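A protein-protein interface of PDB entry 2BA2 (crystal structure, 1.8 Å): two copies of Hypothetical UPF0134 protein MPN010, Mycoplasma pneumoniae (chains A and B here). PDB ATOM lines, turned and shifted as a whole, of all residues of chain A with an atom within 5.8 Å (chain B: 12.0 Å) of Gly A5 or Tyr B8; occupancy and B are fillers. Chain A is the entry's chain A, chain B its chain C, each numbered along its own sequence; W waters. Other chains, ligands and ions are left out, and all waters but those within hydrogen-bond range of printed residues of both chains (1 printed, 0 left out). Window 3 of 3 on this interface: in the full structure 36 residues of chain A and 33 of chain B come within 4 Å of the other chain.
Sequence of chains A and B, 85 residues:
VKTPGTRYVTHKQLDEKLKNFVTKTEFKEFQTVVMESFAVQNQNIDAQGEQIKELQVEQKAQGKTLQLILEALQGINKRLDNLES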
ATOM      1  N   GLY A   5       7.475 -19.032  16.393  1.00  0.00           N
ATOM      2  CA  GLY A   5       8.486 -18.784  15.338  1.00  0.00           C
ATOM      3  C   GLY A   5       9.726 -19.631  15.530  1.00  0.00           C
ATOM      4  O   GLY A   5      10.612 -19.634  14.674  1.00  0.00           O
ATOM      5  N   THR A   6       9.793 -20.360  16.643  1.00  0.00           N
ATOM      6  CA  THR A   6      10.951 -21.205  16.912  1.00  0.00           C
ATOM      7  C   THR A   6      11.042 -22.394  15.953  1.00  0.00           C
ATOM      8  O   THR A   6      12.043 -23.111  15.927  1.00  0.00           O
ATOM      9  CB  THR A   6      10.974 -21.697  18.392  1.00  0.00           C
ATOM     10  OG1 THR A   6      11.360 -23.076  18.440  1.00  0.00           O
ATOM     11  CG2 THR A   6       9.625 -21.508  19.053  1.00  0.00           C
ATOM     12  N   ARG A   7       9.997 -22.598  15.159  1.00  0.00           N
ATOM     13  CA  ARG A   7      10.003 -23.688  14.196  1.00  0.00           C
ATOM     14  C   ARG A   7      10.609 -23.190  12.888  1.00  0.00           C
ATOM     15  O   ARG A   7      10.930 -23.988  12.011  1.00  0.00           O
ATOM     16  CB  ARG A   7       8.582 -24.191  13.915  1.00  0.00           C
ATOM     17  CG  ARG A   7       7.731 -24.478  15.147  1.00  0.00           C
ATOM     18  CD  ARG A   7       7.036 -23.210  15.624  1.00  0.00           C
ATOM     19  NE  ARG A   7       6.197 -22.639  14.576  1.00  0.00           N
ATOM     20  CZ  ARG A   7       5.486 -21.526  14.709  1.00  0.00           C
ATOM     21  NH1 ARG A   7       5.500 -20.850  15.851  1.00  0.00           N
ATOM     22  NH2 ARG A   7       4.762 -21.083  13.692  1.00  0.00           N
ATOM     23  N   TYR A   8      10.789 -21.876  12.778  1.00  0.00           N
ATOM     24  CA  TYR A   8      11.313 -21.271  11.557  1.00  0.00           C
ATOM     25  C   TYR A   8      12.821 -21.077  11.436  1.00  0.00           C
ATOM     26  O   TYR A   8      13.540 -20.927  12.425  1.00  0.00           O
ATOM     27  CB  TYR A   8      10.614 -19.928  11.311  1.00  0.00           C
ATOM     28  CG  TYR A   8       9.115 -20.032  11.180  1.00  0.00           C
ATOM     29  CD1 TYR A   8       8.529 -21.005  10.373  1.00  0.00           C
ATOM     30  CD2 TYR A   8       8.279 -19.140  11.851  1.00  0.00           C
ATOM     31  CE1 TYR A   8       7.142 -21.088  10.238  1.00  0.00           C
ATOM     32  CE2 TYR A   8       6.898 -19.214  11.721  1.00  0.00           C
ATOM     33  CZ  TYR A   8       6.337 -20.190  10.914  1.00  0.00           C
ATOM     34  OH  TYR A   8       4.967 -20.272  10.792  1.00  0.00           O
ATOM     35  N   VAL A   9      13.267 -21.057  10.185  1.00  0.00           N
ATOM     36  CA  VAL A   9      14.667 -20.877   9.822  1.00  0.00           C
ATOM     37  C   VAL A   9      14.994 -19.392   9.708  1.00  0.00           C
ATOM     38  O   VAL A   9      14.295 -18.653   9.011  1.00  0.00           O
ATOM     39  CB  VAL A   9      14.959 -21.512   8.453  1.00  0.00           C
ATOM     40  CG1 VAL A   9      16.397 -21.207   8.020  1.00  0.00           C
ATOM     41  CG2 VAL A   9      14.705 -23.014   8.517  1.00  0.00           C
ATOM     42  N   THR A  10      16.060 -18.963  10.374  1.00  0.00           N
ATOM     43  CA  THR A  10      16.484 -17.566  10.302  1.00  0.00           C
ATOM     44  C   THR A  10      17.412 -17.413   9.094  1.00  0.00           C
ATOM     45  O   THR A  10      17.906 -18.400   8.554  1.00  0.00           O
ATOM     46  CB  THR A  10      17.249 -17.146  11.569  1.00  0.00           C
ATOM     47  OG1 THR A  10      18.449 -17.920  11.678  1.00  0.00           O
ATOM     48  CG2 THR A  10      16.400 -17.373  12.811  1.00  0.00           C
ATOM     49  N   HIS A  11      17.644 -16.177   8.667  1.00  0.00           N
ATOM     50  CA  HIS A  11      18.513 -15.930   7.520  1.00  0.00           C
ATOM     51  C   HIS A  11      19.914 -16.482   7.769  1.00  0.00           C
ATOM     52  O   HIS A  11      20.562 -16.998   6.857  1.00  0.00           O
ATOM     53  CB  HIS A  11      18.583 -14.427   7.238  1.00  0.00           C
ATOM     54  CG  HIS A  11      17.258 -13.818   6.902  1.00  0.00           C
ATOM     55  ND1 HIS A  11      16.593 -14.085   5.723  1.00  0.00           N
ATOM     56  CD2 HIS A  11      16.462 -12.974   7.599  1.00  0.00           C
ATOM     57  CE1 HIS A  11      15.445 -13.431   5.710  1.00  0.00           C
ATOM     58  NE2 HIS A  11      15.341 -12.749   6.837  1.00  0.00           N
ATOM     59  N   GLY B   5       9.012 -11.441   6.650  1.00  0.00           N
ATOM     60  CA  GLY B   5      10.140 -12.288   6.184  1.00  0.00           C
ATOM     61  C   GLY B   5      11.485 -11.738   6.598  1.00  0.00           C
ATOM     62  O   GLY B   5      12.528 -12.231   6.168  1.00  0.00           O
ATOM     63  N   THR B   6      11.462 -10.720   7.450  1.00  0.00           N
ATOM     64  CA  THR B   6      12.687 -10.090   7.907  1.00  0.00           C
ATOM     65  C   THR B   6      13.457 -10.917   8.941  1.00  0.00           C
ATOM     66  O   THR B   6      14.683 -11.003   8.868  1.00  0.00           O
ATOM     67  CB  THR B   6      12.397  -8.674   8.460  1.00  0.00           C
ATOM     68  OG1 THR B   6      13.613  -8.085   8.937  1.00  0.00           O
ATOM     69  CG2 THR B   6      11.382  -8.739   9.582  1.00  0.00           C
ATOM     70  N   ARG B   7      12.768 -11.524   9.905  1.00  0.00           N
ATOM     71  CA  ARG B   7      13.491 -12.327  10.890  1.00  0.00           C
ATOM     72  C   ARG B   7      13.731 -13.730  10.358  1.00  0.00           C
ATOM     73  O   ARG B   7      14.839 -14.269  10.449  1.00  0.00           O
ATOM     74  CB  ARG B   7      12.737 -12.413  12.219  1.00  0.00           C
ATOM     75  CG  ARG B   7      13.555 -13.110  13.304  1.00  0.00           C
ATOM     76  CD  ARG B   7      12.984 -12.915  14.701  1.00  0.00           C
ATOM     77  NE  ARG B   7      13.901 -13.421  15.724  1.00  0.00           N
ATOM     78  CZ  ARG B   7      13.698 -13.328  17.036  1.00  0.00           C
ATOM     79  NH1 ARG B   7      12.602 -12.747  17.506  1.00  0.00           N
ATOM     80  NH2 ARG B   7      14.595 -13.818  17.882  1.00  0.00           N
ATOM     81  N   TYR B   8      12.685 -14.316   9.792  1.00  0.00           N
ATOM     82  CA  TYR B   8      12.779 -15.659   9.256  1.00  0.00           C
ATOM     83  C   TYR B   8      12.728 -15.661   7.733  1.00  0.00           C
ATOM     84  O   TYR B   8      12.211 -14.731   7.102  1.00  0.00           O
ATOM     85  CB  TYR B   8      11.659 -16.519   9.846  1.00  0.00           C
ATOM     86  CG  TYR B   8      11.707 -16.559  11.360  1.00  0.00           C
ATOM     87  CD1 TYR B   8      12.754 -17.197  12.026  1.00  0.00           C
ATOM     88  CD2 TYR B   8      10.737 -15.908  12.128  1.00  0.00           C
ATOM     89  CE1 TYR B   8      12.841 -17.185  13.418  1.00  0.00           C
ATOM     90  CE2 TYR B   8      10.816 -15.887  13.522  1.00  0.00           C
ATOM     91  CZ  TYR B   8      11.869 -16.526  14.156  1.00  0.00           C
ATOM     92  OH  TYR B   8      11.963 -16.500  15.528  1.00  0.00           O
ATOM     93  N   VAL B   9      13.286 -16.714   7.153  1.00  0.00           N
ATOM     94  CA  VAL B   9      13.325 -16.875   5.710  1.00  0.00           C
ATOM     95  C   VAL B   9      11.943 -17.224   5.183  1.00  0.00           C
ATOM     96  O   VAL B   9      11.242 -18.044   5.767  1.00  0.00           O
ATOM     97  CB  VAL B   9      14.300 -18.006   5.324  1.00  0.00           C
ATOM     98  CG1 VAL B   9      14.304 -18.213   3.813  1.00  0.00           C
ATOM     99  CG2 VAL B   9      15.691 -17.664   5.821  1.00  0.00           C
ATOM    100  N   THR B  10      11.544 -16.601   4.081  1.00  0.00           N
ATOM    101  CA  THR B  10      10.250 -16.911   3.491  1.00  0.00           C
ATOM    102  C   THR B  10      10.483 -17.899   2.357  1.00  0.00           C
ATOM    103  O   THR B  10      11.592 -18.027   1.864  1.00  0.00           O
ATOM    104  CB  THR B  10       9.573 -15.663   2.911  1.00  0.00           C
ATOM    105  OG1 THR B  10      10.242 -15.271   1.705  1.00  0.00           O
ATOM    106  CG2 THR B  10       9.631 -14.527   3.909  1.00  0.00           C
ATOM    107  N   HIS B  11       9.430 -18.585   1.941  1.00  0.00           N
ATOM    108  CA  HIS B  11       9.544 -19.558   0.865  1.00  0.00           C
ATOM    109  C   HIS B  11       9.993 -18.922  -0.448  1.00  0.00           C
ATOM    110  O   HIS B  11      10.649 -19.567  -1.260  1.00  0.00           O
ATOM    111  CB  HIS B  11       8.210 -20.282   0.683  1.00  0.00           C
ATOM    112  CG  HIS B  11       7.945 -21.308   1.738  1.00  0.00           C
ATOM    113  ND1 HIS B  11       8.552 -22.546   1.739  1.00  0.00           N
ATOM    114  CD2 HIS B  11       7.195 -21.257   2.865  1.00  0.00           C
ATOM    115  CE1 HIS B  11       8.191 -23.211   2.821  1.00  0.00           C
ATOM    116  NE2 HIS B  11       7.368 -22.451   3.522  1.00  0.00           N
ATOM    117  N   LYS B  12       9.649 -17.656  -0.648  1.00  0.00           N
ATOM    118  CA  LYS B  12      10.042 -16.967  -1.871  1.00  0.00           C
ATOM    119  C   LYS B  12      11.537 -16.691  -1.845  1.00  0.00           C
ATOM    120  O   LYS B  12      12.223 -16.839  -2.850  1.00  0.00           O
ATOM    121  CB  LYS B  12       9.291 -15.641  -2.021  1.00  0.00           C
ATOM    122  CG  LYS B  12       9.308 -15.107  -3.450  1.00  0.00           C
ATOM    123  CD  LYS B  12       8.953 -13.630  -3.528  1.00  0.00           C
ATOM    124  CE  LYS B  12      10.149 -12.759  -3.163  1.00  0.00           C
ATOM    125  NZ  LYS B  12      11.295 -12.985  -4.095  1.00  0.00           N
ATOM    126  N   GLN B  13      12.037 -16.287  -0.684  1.00  0.00           N
ATOM    127  CA  GLN B  13      13.455 -15.984  -0.533  1.00  0.00           C
ATOM    128  C   GLN B  13      14.301 -17.245  -0.661  1.00  0.00           C
ATOM    129  O   GLN B  13      15.406 -17.205  -1.194  1.00  0.00           O
ATOM    130  CB  GLN B  13      13.709 -15.322   0.818  1.00  0.00           C
ATOM    131  CG  GLN B  13      12.916 -14.041   1.015  1.00  0.00           C
ATOM    132  CD  GLN B  13      13.111 -13.449   2.390  1.00  0.00           C
ATOM    133  OE1 GLN B  13      13.019 -14.151   3.394  1.00  0.00           O
ATOM    134  NE2 GLN B  13      13.371 -12.146   2.447  1.00  0.00           N
ATOM    135  N   LEU B  14      13.785 -18.367  -0.177  1.00  0.00           N
ATOM    136  CA  LEU B  14      14.521 -19.628  -0.273  1.00  0.00           C
ATOM    137  C   LEU B  14      14.593 -20.102  -1.729  1.00  0.00           C
ATOM    138  O   LEU B  14      15.654 -20.509  -2.223  1.00  0.00           O
ATOM    139  CB  LEU B  14      13.845 -20.698   0.586  1.00  0.00           C
ATOM    140  CG  LEU B  14      14.450 -22.104   0.514  1.00  0.00           C
ATOM    141  CD1 LEU B  14      15.938 -22.060   0.873  1.00  0.00           C
ATOM    142  CD2 LEU B  14      13.678 -23.034   1.459  1.00  0.00           C
ATOM    143  N   ASP B  15      13.456 -20.057  -2.412  1.00  0.00           N
ATOM    144  CA  ASP B  15      13.393 -20.471  -3.809  1.00  0.00           C
ATOM    145  C   ASP B  15      14.361 -19.642  -4.636  1.00  0.00           C
ATOM    146  O   ASP B  15      15.050 -20.166  -5.511  1.00  0.00           O
ATOM    147  CB  ASP B  15      11.973 -20.299  -4.348  1.00  0.00           C
ATOM    148  CG  ASP B  15      11.027 -21.370  -3.845  1.00  0.00           C
ATOM    149  OD1 ASP B  15       9.798 -21.193  -3.989  1.00  0.00           O
ATOM    150  OD2 ASP B  15      11.514 -22.393  -3.313  1.00  0.00           O
ATOM    151  N   GLU B  16      14.408 -18.347  -4.344  1.00  0.00           N
ATOM    152  CA  GLU B  16      15.297 -17.427  -5.038  1.00  0.00           C
ATOM    153  C   GLU B  16      16.748 -17.823  -4.768  1.00  0.00           C
ATOM    154  O   GLU B  16      17.582 -17.818  -5.666  1.00  0.00           O
ATOM    155  CB  GLU B  16      15.033 -15.995  -4.556  1.00  0.00           C
ATOM    156  CG  GLU B  16      15.920 -14.929  -5.182  1.00  0.00           C
ATOM    157  CD  GLU B  16      17.352 -14.981  -4.680  1.00  0.00           C
ATOM    158  OE1 GLU B  16      17.563 -14.837  -3.455  1.00  0.00           O
ATOM    159  OE2 GLU B  16      18.268 -15.165  -5.511  1.00  0.00           O
ATOM    160  N   LYS B  17      17.035 -18.160  -3.517  1.00  0.00           N
ATOM    161  CA  LYS B  17      18.375 -18.572  -3.116  1.00  0.00           C
ATOM    162  C   LYS B  17      18.777 -19.881  -3.786  1.00  0.00           C
ATOM    163  O   LYS B  17      19.897 -20.023  -4.271  1.00  0.00           O
ATOM    164  CB  LYS B  17      18.437 -18.760  -1.598  1.00  0.00           C
ATOM    165  CG  LYS B  17      19.264 -17.728  -0.854  1.00  0.00           C
ATOM    166  CD  LYS B  17      18.505 -16.441  -0.606  1.00  0.00           C
ATOM    167  CE  LYS B  17      19.300 -15.515   0.309  1.00  0.00           C
ATOM    168  NZ  LYS B  17      18.511 -14.320   0.727  1.00  0.00           N
HETATM  169  O   HOH W   1      18.308 -15.103   3.502  1.00  0.00           O
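Among the printed residues, pairs that only touch across the chains: Gly A5 with Tyr B8, Tyr A8 with Tyr B8, Val A9 with Tyr B8, Thr A10 with Arg B7, Thr A10 with Tyr B8, Thr A10 with Val B9, His A11 with Arg B7, His A11 with Tyr B8, His A11 with Val B9 and His A11 with Gln B13.
The backbone carbonyl oxygen (O) of Gly B5 sits close to the side-chain amide oxygen (OE1) of Gln B13, at 3.4 Å. The backbone NH (N) of Thr B10 lies within hydrogen-bond range of the side-chain amide oxygen (OE1) of Gln B13, at 2.9 Å. The backbone NH (N) of Gly A5 sits close to the guanidinium group (NH1) of Arg A7 (2.7 Å). The guanidinium group of Arg A7 is in hydrogen-bond range of the side-chain hydroxyl of Tyr A8, 3.0 Å away.
Of the 7 printed residues of chain A, 5 touch a printed residue of chain B. Printed residues of chain A that touch a printed residue of chain B: Gly A5, Tyr A8, Val A9, Thr A10 and His A11. Hydrophobic or aromatic side chains of chain A that line the printed part of chain B: Tyr A8 and His A11. Of the 13 printed residues of chain B, 6 touch a printed residue of chain A. Printed residues of chain B that touch a printed residue of chain A: Gly B5, Thr B6, Arg B7, Tyr B8, Val B9 and Gln B13. Hydrophobic or aromatic side chains of chain B that line the printed part of chain A: Tyr B8 and Val B9.
Gly A5 touches Tyr B8, but with the chains exchanged Tyr A8 does not touch Gly B5 (9.1 Å). Val A9 touches Tyr B8, but with the chains exchanged Tyr A8 does not touch Val B9 (5.9 Å). Thr A10 touches Arg B7, but with the chains exchanged Arg A7 does not touch Thr B10 (10.9 Å). His A11 touches Thr B6, but with the chains exchanged Thr A6 does not touch His B11 (13.0 Å). Positions printed for both chains: 5, 6, 7, 8, 9, 10 and 11. Of the 13 pairs that touch across the chains among the printed residues, 2 have their exchanged pair printed and touching as well.
Water W1 bridges the side-chain amino group (NZ) of Lys B17 (2.9 Å) and a ring nitrogen (ND1) of His A11 (3.0 Å).
Gly A5 touches one residue of chain B. No residue of chain B comes within 4 Å of Arg A7. Tyr A8 touches just one residue of chain B: Tyr B8 (3.5 Å). Val A9 touches two residues of chain B. Of the printed residues of chain A, Gln B13 touches His A11. Of the printed residues of chain B, His A11 touches Gly B5, Thr B6, Arg B7, Tyr B8, Val B9 and Gln B13. Printed residues of chain A within 4 Å of Arg B7: Thr A10 (3.7 Å) and His A11 (3.5 Å). Glu B16 touches none of the printed residues of chain A. The nearest residue of chain B that does not touch Gly A5 is Arg B7 (7.1 Å). The nearest printed residue of chain A that does not touch Val B9 is Tyr A8 (5.9 Å).
The backbone carbonyl oxygen of Val A9 sits at hydrogen-bond distance from the backbone NH of Val B9, 2.9 Å away. The backbone carbonyl oxygen of Gly B5 is in hydrogen-bond range of a ring nitrogen (NE2) of His A11. A ring nitrogen (NE2) of His A11 sits at hydrogen-bond distance from the backbone carbonyl oxygen of Thr B6, at 2.8 Å.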
